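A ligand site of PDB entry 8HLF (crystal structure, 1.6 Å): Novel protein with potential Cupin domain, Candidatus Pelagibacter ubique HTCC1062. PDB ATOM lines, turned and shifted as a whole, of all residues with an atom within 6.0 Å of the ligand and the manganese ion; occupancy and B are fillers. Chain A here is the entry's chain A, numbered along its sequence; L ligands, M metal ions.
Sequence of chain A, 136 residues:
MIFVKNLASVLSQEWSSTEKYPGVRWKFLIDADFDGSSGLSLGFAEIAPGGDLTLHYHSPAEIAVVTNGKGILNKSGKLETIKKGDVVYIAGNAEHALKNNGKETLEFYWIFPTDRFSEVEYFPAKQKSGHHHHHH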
ATOM      1  N   TYR A  21      26.878   2.839  18.291  1.00  0.00           N
ATOM      2  CA  TYR A  21      26.758   3.260  16.897  1.00  0.00           C
ATOM      3  C   TYR A  21      25.874   4.504  16.843  1.00  0.00           C
ATOM      4  O   TYR A  21      24.669   4.417  16.585  1.00  0.00           O
ATOM      5  CB  TYR A  21      26.172   2.148  16.014  1.00  0.00           C
ATOM      6  CG  TYR A  21      26.975   0.867  16.011  1.00  0.00           C
ATOM      7  CD1 TYR A  21      28.373   0.887  16.127  1.00  0.00           C
ATOM      8  CD2 TYR A  21      26.354  -0.366  15.872  1.00  0.00           C
ATOM      9  CE1 TYR A  21      29.103  -0.289  16.130  1.00  0.00           C
ATOM     10  CE2 TYR A  21      27.080  -1.550  15.870  1.00  0.00           C
ATOM     11  CZ  TYR A  21      28.456  -1.504  15.986  1.00  0.00           C
ATOM     12  OH  TYR A  21      29.178  -2.672  15.982  1.00  0.00           O
ATOM     13  N   VAL A  24      22.767   5.608  14.183  1.00  0.00           N
ATOM     14  CA  VAL A  24      22.460   4.414  13.406  1.00  0.00           C
ATOM     15  C   VAL A  24      21.196   3.773  13.980  1.00  0.00           C
ATOM     16  O   VAL A  24      21.084   3.602  15.200  1.00  0.00           O
ATOM     17  CB  VAL A  24      23.628   3.409  13.417  1.00  0.00           C
ATOM     18  CG1 VAL A  24      23.307   2.189  12.551  1.00  0.00           C
ATOM     19  CG2 VAL A  24      24.920   4.085  12.925  1.00  0.00           C
ATOM     20  N   ARG A  25      20.254   3.418  13.104  1.00  0.00           N
ATOM     21  CA  ARG A  25      19.062   2.714  13.534  1.00  0.00           C
ATOM     22  C   ARG A  25      18.654   1.737  12.439  1.00  0.00           C
ATOM     23  O   ARG A  25      18.983   1.930  11.261  1.00  0.00           O
ATOM     24  CB  ARG A  25      17.909   3.665  13.867  1.00  0.00           C
ATOM     25  CG  ARG A  25      17.388   4.489  12.707  1.00  0.00           C
ATOM     26  CD  ARG A  25      16.252   5.374  13.144  1.00  0.00           C
ATOM     27  NE  ARG A  25      15.543   5.933  12.001  1.00  0.00           N
ATOM     28  CZ  ARG A  25      14.450   6.684  12.106  1.00  0.00           C
ATOM     29  NH1 ARG A  25      13.862   7.151  11.017  1.00  0.00           N
ATOM     30  NH2 ARG A  25      13.959   6.970  13.302  1.00  0.00           N
ATOM     31  N   TRP A  26      17.957   0.675  12.825  1.00  0.00           N
ATOM     32  CA  TRP A  26      17.666  -0.379  11.864  1.00  0.00           C
ATOM     33  C   TRP A  26      16.377  -1.101  12.223  1.00  0.00           C
ATOM     34  O   TRP A  26      15.889  -1.049  13.350  1.00  0.00           O
ATOM     35  CB  TRP A  26      18.813  -1.396  11.771  1.00  0.00           C
ATOM     36  CG  TRP A  26      19.205  -2.019  13.080  1.00  0.00           C
ATOM     37  CD1 TRP A  26      18.748  -3.204  13.602  1.00  0.00           C
ATOM     38  CD2 TRP A  26      20.159  -1.517  14.023  1.00  0.00           C
ATOM     39  NE1 TRP A  26      19.355  -3.455  14.810  1.00  0.00           N
ATOM     40  CE2 TRP A  26      20.222  -2.432  15.091  1.00  0.00           C
ATOM     41  CE3 TRP A  26      20.967  -0.376  14.061  1.00  0.00           C
ATOM     42  CZ2 TRP A  26      21.052  -2.245  16.192  1.00  0.00           C
ATOM     43  CZ3 TRP A  26      21.788  -0.185  15.164  1.00  0.00           C
ATOM     44  CH2 TRP A  26      21.830  -1.113  16.209  1.00  0.00           C
ATOM     45  N   PHE A  28      14.373  -5.076  11.129  1.00  0.00           N
ATOM     46  CA  PHE A  28      14.535  -6.414  10.585  1.00  0.00           C
ATOM     47  C   PHE A  28      13.359  -6.733   9.676  1.00  0.00           C
ATOM     48  O   PHE A  28      12.212  -6.754  10.121  1.00  0.00           O
ATOM     49  CB  PHE A  28      14.628  -7.428  11.715  1.00  0.00           C
ATOM     50  CG  PHE A  28      15.658  -7.072  12.733  1.00  0.00           C
ATOM     51  CD1 PHE A  28      16.999  -7.262  12.457  1.00  0.00           C
ATOM     52  CD2 PHE A  28      15.301  -6.528  13.949  1.00  0.00           C
ATOM     53  CE1 PHE A  28      17.971  -6.931  13.382  1.00  0.00           C
ATOM     54  CE2 PHE A  28      16.264  -6.193  14.875  1.00  0.00           C
ATOM     55  CZ  PHE A  28      17.606  -6.402  14.587  1.00  0.00           C
ATOM     56  N   PHE A  44      17.144  -3.326   7.278  1.00  0.00           N
ATOM     57  CA  PHE A  44      17.260  -2.006   6.663  1.00  0.00           C
ATOM     58  C   PHE A  44      17.813  -1.059   7.701  1.00  0.00           C
ATOM     59  O   PHE A  44      17.326  -1.029   8.839  1.00  0.00           O
ATOM     60  CB  PHE A  44      15.907  -1.501   6.164  1.00  0.00           C
ATOM     61  CG  PHE A  44      15.950  -0.114   5.592  1.00  0.00           C
ATOM     62  CD1 PHE A  44      16.538   0.128   4.360  1.00  0.00           C
ATOM     63  CD2 PHE A  44      15.409   0.957   6.301  1.00  0.00           C
ATOM     64  CE1 PHE A  44      16.582   1.431   3.832  1.00  0.00           C
ATOM     65  CE2 PHE A  44      15.443   2.245   5.762  1.00  0.00           C
ATOM     66  CZ  PHE A  44      16.031   2.481   4.539  1.00  0.00           C
ATOM     67  N   ALA A  45      18.830  -0.290   7.322  1.00  0.00           N
ATOM     68  CA  ALA A  45      19.519   0.600   8.250  1.00  0.00           C
ATOM     69  C   ALA A  45      19.527   2.020   7.717  1.00  0.00           C
ATOM     70  O   ALA A  45      19.643   2.242   6.517  1.00  0.00           O
ATOM     71  CB  ALA A  45      20.954   0.134   8.502  1.00  0.00           C
ATOM     72  N   LEU A  53      28.790   3.890  11.985  1.00  0.00           N
ATOM     73  CA  LEU A  53      28.837   2.465  12.301  1.00  0.00           C
ATOM     74  C   LEU A  53      30.306   2.119  12.406  1.00  0.00           C
ATOM     75  O   LEU A  53      30.994   1.957  11.392  1.00  0.00           O
ATOM     76  CB  LEU A  53      28.115   1.668  11.224  1.00  0.00           C
ATOM     77  CG  LEU A  53      28.156   0.140  11.301  1.00  0.00           C
ATOM     78  CD1 LEU A  53      27.623  -0.325  12.641  1.00  0.00           C
ATOM     79  CD2 LEU A  53      27.346  -0.446  10.164  1.00  0.00           C
ATOM     80  N   HIS A  56      34.256  -2.847  12.963  1.00  0.00           N
ATOM     81  CA  HIS A  56      33.820  -4.076  13.613  1.00  0.00           C
ATOM     82  C   HIS A  56      33.952  -5.216  12.621  1.00  0.00           C
ATOM     83  O   HIS A  56      34.240  -5.014  11.443  1.00  0.00           O
ATOM     84  CB  HIS A  56      32.362  -3.966  14.107  1.00  0.00           C
ATOM     85  CG  HIS A  56      31.370  -3.969  12.989  1.00  0.00           C
ATOM     86  ND1 HIS A  56      31.013  -2.810  12.321  1.00  0.00           N
ATOM     87  CD2 HIS A  56      30.681  -4.970  12.405  1.00  0.00           C
ATOM     88  CE1 HIS A  56      30.134  -3.105  11.383  1.00  0.00           C
ATOM     89  NE2 HIS A  56      29.917  -4.405  11.398  1.00  0.00           N
ATOM     90  N   TYR A  57      33.758  -6.430  13.124  1.00  0.00           N
ATOM     91  CA  TYR A  57      33.732  -7.588  12.253  1.00  0.00           C
ATOM     92  C   TYR A  57      32.804  -8.642  12.860  1.00  0.00           C
ATOM     93  O   TYR A  57      32.437  -8.582  14.031  1.00  0.00           O
ATOM     94  CB  TYR A  57      35.129  -8.171  12.019  1.00  0.00           C
ATOM     95  CG  TYR A  57      35.834  -8.696  13.252  1.00  0.00           C
ATOM     96  CD1 TYR A  57      36.521  -7.829  14.096  1.00  0.00           C
ATOM     97  CD2 TYR A  57      35.826 -10.045  13.559  1.00  0.00           C
ATOM     98  CE1 TYR A  57      37.169  -8.297  15.215  1.00  0.00           C
ATOM     99  CE2 TYR A  57      36.481 -10.527  14.694  1.00  0.00           C
ATOM    100  CZ  TYR A  57      37.149  -9.644  15.510  1.00  0.00           C
ATOM    101  OH  TYR A  57      37.806 -10.097  16.639  1.00  0.00           O
ATOM    102  N   HIS A  58      32.449  -9.610  12.023  1.00  0.00           N
ATOM    103  CA  HIS A  58      31.618 -10.743  12.409  1.00  0.00           C
ATOM    104  C   HIS A  58      31.891 -11.878  11.449  1.00  0.00           C
ATOM    105  O   HIS A  58      32.264 -11.644  10.291  1.00  0.00           O
ATOM    106  CB  HIS A  58      30.131 -10.370  12.399  1.00  0.00           C
ATOM    107  CG  HIS A  58      29.796  -9.320  11.399  1.00  0.00           C
ATOM    108  ND1 HIS A  58      30.007  -9.490  10.047  1.00  0.00           N
ATOM    109  CD2 HIS A  58      29.264  -8.076  11.544  1.00  0.00           C
ATOM    110  CE1 HIS A  58      29.649  -8.388   9.404  1.00  0.00           C
ATOM    111  NE2 HIS A  58      29.192  -7.526  10.292  1.00  0.00           N
ATOM    112  N   GLU A  62      28.869 -10.593   4.489  1.00  0.00           N
ATOM    113  CA  GLU A  62      27.774  -9.637   4.528  1.00  0.00           C
ATOM    114  C   GLU A  62      27.705  -8.913   3.193  1.00  0.00           C
ATOM    115  O   GLU A  62      28.733  -8.618   2.579  1.00  0.00           O
ATOM    116  CB  GLU A  62      27.968  -8.606   5.663  1.00  0.00           C
ATOM    117  CG  GLU A  62      26.879  -7.531   5.738  1.00  0.00           C
ATOM    118  CD  GLU A  62      27.206  -6.407   6.723  1.00  0.00           C
ATOM    119  OE1 GLU A  62      28.091  -6.577   7.595  1.00  0.00           O
ATOM    120  OE2 GLU A  62      26.596  -5.320   6.612  1.00  0.00           O
ATOM    121  N   ILE A  90      31.362  -7.809   1.969  1.00  0.00           N
ATOM    122  CA  ILE A  90      32.270  -7.778   3.116  1.00  0.00           C
ATOM    123  C   ILE A  90      32.551  -9.227   3.507  1.00  0.00           C
ATOM    124  O   ILE A  90      31.656  -9.933   3.986  1.00  0.00           O
ATOM    125  CB  ILE A  90      31.670  -7.010   4.304  1.00  0.00           C
ATOM    126  CG1 ILE A  90      31.299  -5.594   3.859  1.00  0.00           C
ATOM    127  CG2 ILE A  90      32.633  -7.013   5.474  1.00  0.00           C
ATOM    128  CD1 ILE A  90      30.110  -5.048   4.567  1.00  0.00           C
ATOM    129  N   HIS A  96      35.355  -3.636   9.108  1.00  0.00           N
ATOM    130  CA  HIS A  96      34.699  -2.633   8.272  1.00  0.00           C
ATOM    131  C   HIS A  96      33.937  -1.627   9.124  1.00  0.00           C
ATOM    132  O   HIS A  96      33.551  -1.904  10.256  1.00  0.00           O
ATOM    133  CB  HIS A  96      33.758  -3.269   7.239  1.00  0.00           C
ATOM    134  CG  HIS A  96      32.702  -4.142   7.844  1.00  0.00           C
ATOM    135  ND1 HIS A  96      32.985  -5.363   8.430  1.00  0.00           N
ATOM    136  CD2 HIS A  96      31.367  -3.964   7.973  1.00  0.00           C
ATOM    137  CE1 HIS A  96      31.861  -5.903   8.873  1.00  0.00           C
ATOM    138  NE2 HIS A  96      30.862  -5.073   8.603  1.00  0.00           N
ATOM    139  N   PHE A 108      20.604   1.782   3.696  1.00  0.00           N
ATOM    140  CA  PHE A 108      21.000   0.560   3.018  1.00  0.00           C
ATOM    141  C   PHE A 108      20.300  -0.648   3.622  1.00  0.00           C
ATOM    142  O   PHE A 108      19.925  -0.654   4.800  1.00  0.00           O
ATOM    143  CB  PHE A 108      22.526   0.350   3.071  1.00  0.00           C
ATOM    144  CG  PHE A 108      23.102   0.264   4.456  1.00  0.00           C
ATOM    145  CD1 PHE A 108      23.396   1.405   5.165  1.00  0.00           C
ATOM    146  CD2 PHE A 108      23.376  -0.973   5.031  1.00  0.00           C
ATOM    147  CE1 PHE A 108      23.933   1.334   6.460  1.00  0.00           C
ATOM    148  CE2 PHE A 108      23.928  -1.054   6.310  1.00  0.00           C
ATOM    149  CZ  PHE A 108      24.197   0.105   7.015  1.00  0.00           C
ATOM    150  N   TRP A 110      21.123  -4.634   4.573  1.00  0.00           N
ATOM    151  CA  TRP A 110      22.181  -5.613   4.738  1.00  0.00           C
ATOM    152  C   TRP A 110      21.590  -7.007   4.635  1.00  0.00           C
ATOM    153  O   TRP A 110      20.393  -7.218   4.890  1.00  0.00           O
ATOM    154  CB  TRP A 110      22.917  -5.464   6.073  1.00  0.00           C
ATOM    155  CG  TRP A 110      22.196  -6.058   7.229  1.00  0.00           C
ATOM    156  CD1 TRP A 110      22.215  -7.358   7.639  1.00  0.00           C
ATOM    157  CD2 TRP A 110      21.342  -5.362   8.142  1.00  0.00           C
ATOM    158  NE1 TRP A 110      21.431  -7.526   8.748  1.00  0.00           N
ATOM    159  CE2 TRP A 110      20.869  -6.312   9.082  1.00  0.00           C
ATOM    160  CE3 TRP A 110      20.899  -4.038   8.253  1.00  0.00           C
ATOM    161  CZ2 TRP A 110      20.010  -5.975  10.120  1.00  0.00           C
ATOM    162  CZ3 TRP A 110      20.041  -3.696   9.281  1.00  0.00           C
ATOM    163  CH2 TRP A 110      19.612  -4.667  10.215  1.00  0.00           C
ATOM    164  N   PHE A 112      22.774 -11.176   5.513  1.00  0.00           N
ATOM    165  CA  PHE A 112      23.678 -12.175   6.056  1.00  0.00           C
ATOM    166  C   PHE A 112      23.209 -13.557   5.614  1.00  0.00           C
ATOM    167  O   PHE A 112      22.010 -13.785   5.459  1.00  0.00           O
ATOM    168  CB  PHE A 112      23.688 -12.161   7.590  1.00  0.00           C
ATOM    169  CG  PHE A 112      24.438 -11.018   8.209  1.00  0.00           C
ATOM    170  CD1 PHE A 112      25.822 -10.920   8.063  1.00  0.00           C
ATOM    171  CD2 PHE A 112      23.777 -10.079   8.975  1.00  0.00           C
ATOM    172  CE1 PHE A 112      26.512  -9.876   8.662  1.00  0.00           C
ATOM    173  CE2 PHE A 112      24.467  -9.034   9.574  1.00  0.00           C
ATOM    174  CZ  PHE A 112      25.845  -8.942   9.401  1.00  0.00           C
ATOM    175  N   PHE A 117      19.377 -12.291  12.534  1.00  0.00           N
ATOM    176  CA  PHE A 117      20.400 -11.326  12.929  1.00  0.00           C
ATOM    177  C   PHE A 117      21.062 -11.726  14.232  1.00  0.00           C
ATOM    178  O   PHE A 117      22.266 -11.524  14.419  1.00  0.00           O
ATOM    179  CB  PHE A 117      19.764  -9.941  13.052  1.00  0.00           C
ATOM    180  CG  PHE A 117      20.722  -8.849  13.432  1.00  0.00           C
ATOM    181  CD1 PHE A 117      21.637  -8.372  12.525  1.00  0.00           C
ATOM    182  CD2 PHE A 117      20.672  -8.287  14.699  1.00  0.00           C
ATOM    183  CE1 PHE A 117      22.507  -7.359  12.859  1.00  0.00           C
ATOM    184  CE2 PHE A 117      21.536  -7.268  15.048  1.00  0.00           C
ATOM    185  CZ  PHE A 117      22.455  -6.802  14.135  1.00  0.00           C
ATOM    186  N   TYR A 122      28.903  -9.648  16.877  1.00  0.00           N
ATOM    187  CA  TYR A 122      29.722  -8.513  16.480  1.00  0.00           C
ATOM    188  C   TYR A 122      30.911  -8.337  17.411  1.00  0.00           C
ATOM    189  O   TYR A 122      30.775  -8.428  18.593  1.00  0.00           O
ATOM    190  CB  TYR A 122      28.936  -7.208  16.452  1.00  0.00           C
ATOM    191  CG  TYR A 122      28.017  -6.986  15.255  1.00  0.00           C
ATOM    192  CD1 TYR A 122      27.055  -7.892  14.938  1.00  0.00           C
ATOM    193  CD2 TYR A 122      28.101  -5.853  14.490  1.00  0.00           C
ATOM    194  CE1 TYR A 122      26.249  -7.686  13.887  1.00  0.00           C
ATOM    195  CE2 TYR A 122      27.285  -5.640  13.418  1.00  0.00           C
ATOM    196  CZ  TYR A 122      26.340  -6.567  13.137  1.00  0.00           C
ATOM    197  OH  TYR A 122      25.538  -6.403  12.086  1.00  0.00           O
HETATM  198  O1  LIG L   1      27.392  -3.763   8.715  1.00  0.00           O
HETATM  199  C1  LIG L   1      26.606  -4.338   9.522  1.00  0.00           C
HETATM  200  C2  LIG L   1      25.298  -3.667   9.926  1.00  0.00           C
HETATM  201  O2  LIG L   1      26.898  -5.474   9.972  1.00  0.00           O
HETATM  202  C3  LIG L   1      25.252  -3.535  11.452  1.00  0.00           C
HETATM  203  S1  LIG L   1      23.547  -3.199  11.978  1.00  0.00           S
HETATM  204  C4  LIG L   1      22.546  -4.709  11.799  1.00  0.00           C
HETATM  205  C5  LIG L   1      22.844  -1.881  10.949  1.00  0.00           C
HETATM  206  O3  LIG L   1      23.540  -2.778  13.378  1.00  0.00           O
HETATM  207 MN    MN M   1      28.966  -5.482   9.585  1.00  0.00          MN
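The manganese ion is bound by O2 of the ligand (2.1 Å), NE2 of His 96 (2.2 Å), NE2 of His 58 (2.2 Å), NE2 of His 56 (2.3 Å), OE1 of Glu 62 (2.4 Å) and O1 of the ligand (2.5 Å).
N of Ala 45 lies within hydrogen-bond range of O of Phe 108 (2.8 Å).
The backbone carbonyl oxygen (O) of Glu 62 sits at hydrogen-bond distance from the backbone NH (N) of Ile 90.
Residues that only touch the ligand: Trp 26 (3.6 Å), Ala 45 (3.7 Å), Leu 53 (3.6 Å), Trp 110 (3.3 Å), Phe 112 (3.7 Å) and Phe 117 (2.9 Å).
Hydrophobic or aromatic side chains that line the ligand: Trp 26, Ala 45, Leu 53, His 56, His 58, Trp 110, Phe 112, Phe 117 and Tyr 122.
11 residues have an atom within 4 Å of the ligand: Trp 26, Ala 45, Leu 53, His 56, His 58, Glu 62, His 96, Trp 110, Phe 112, Phe 117 and Tyr 122.
OH of Tyr 122 sits close to O2 of the ligand, at 2.7 Å.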
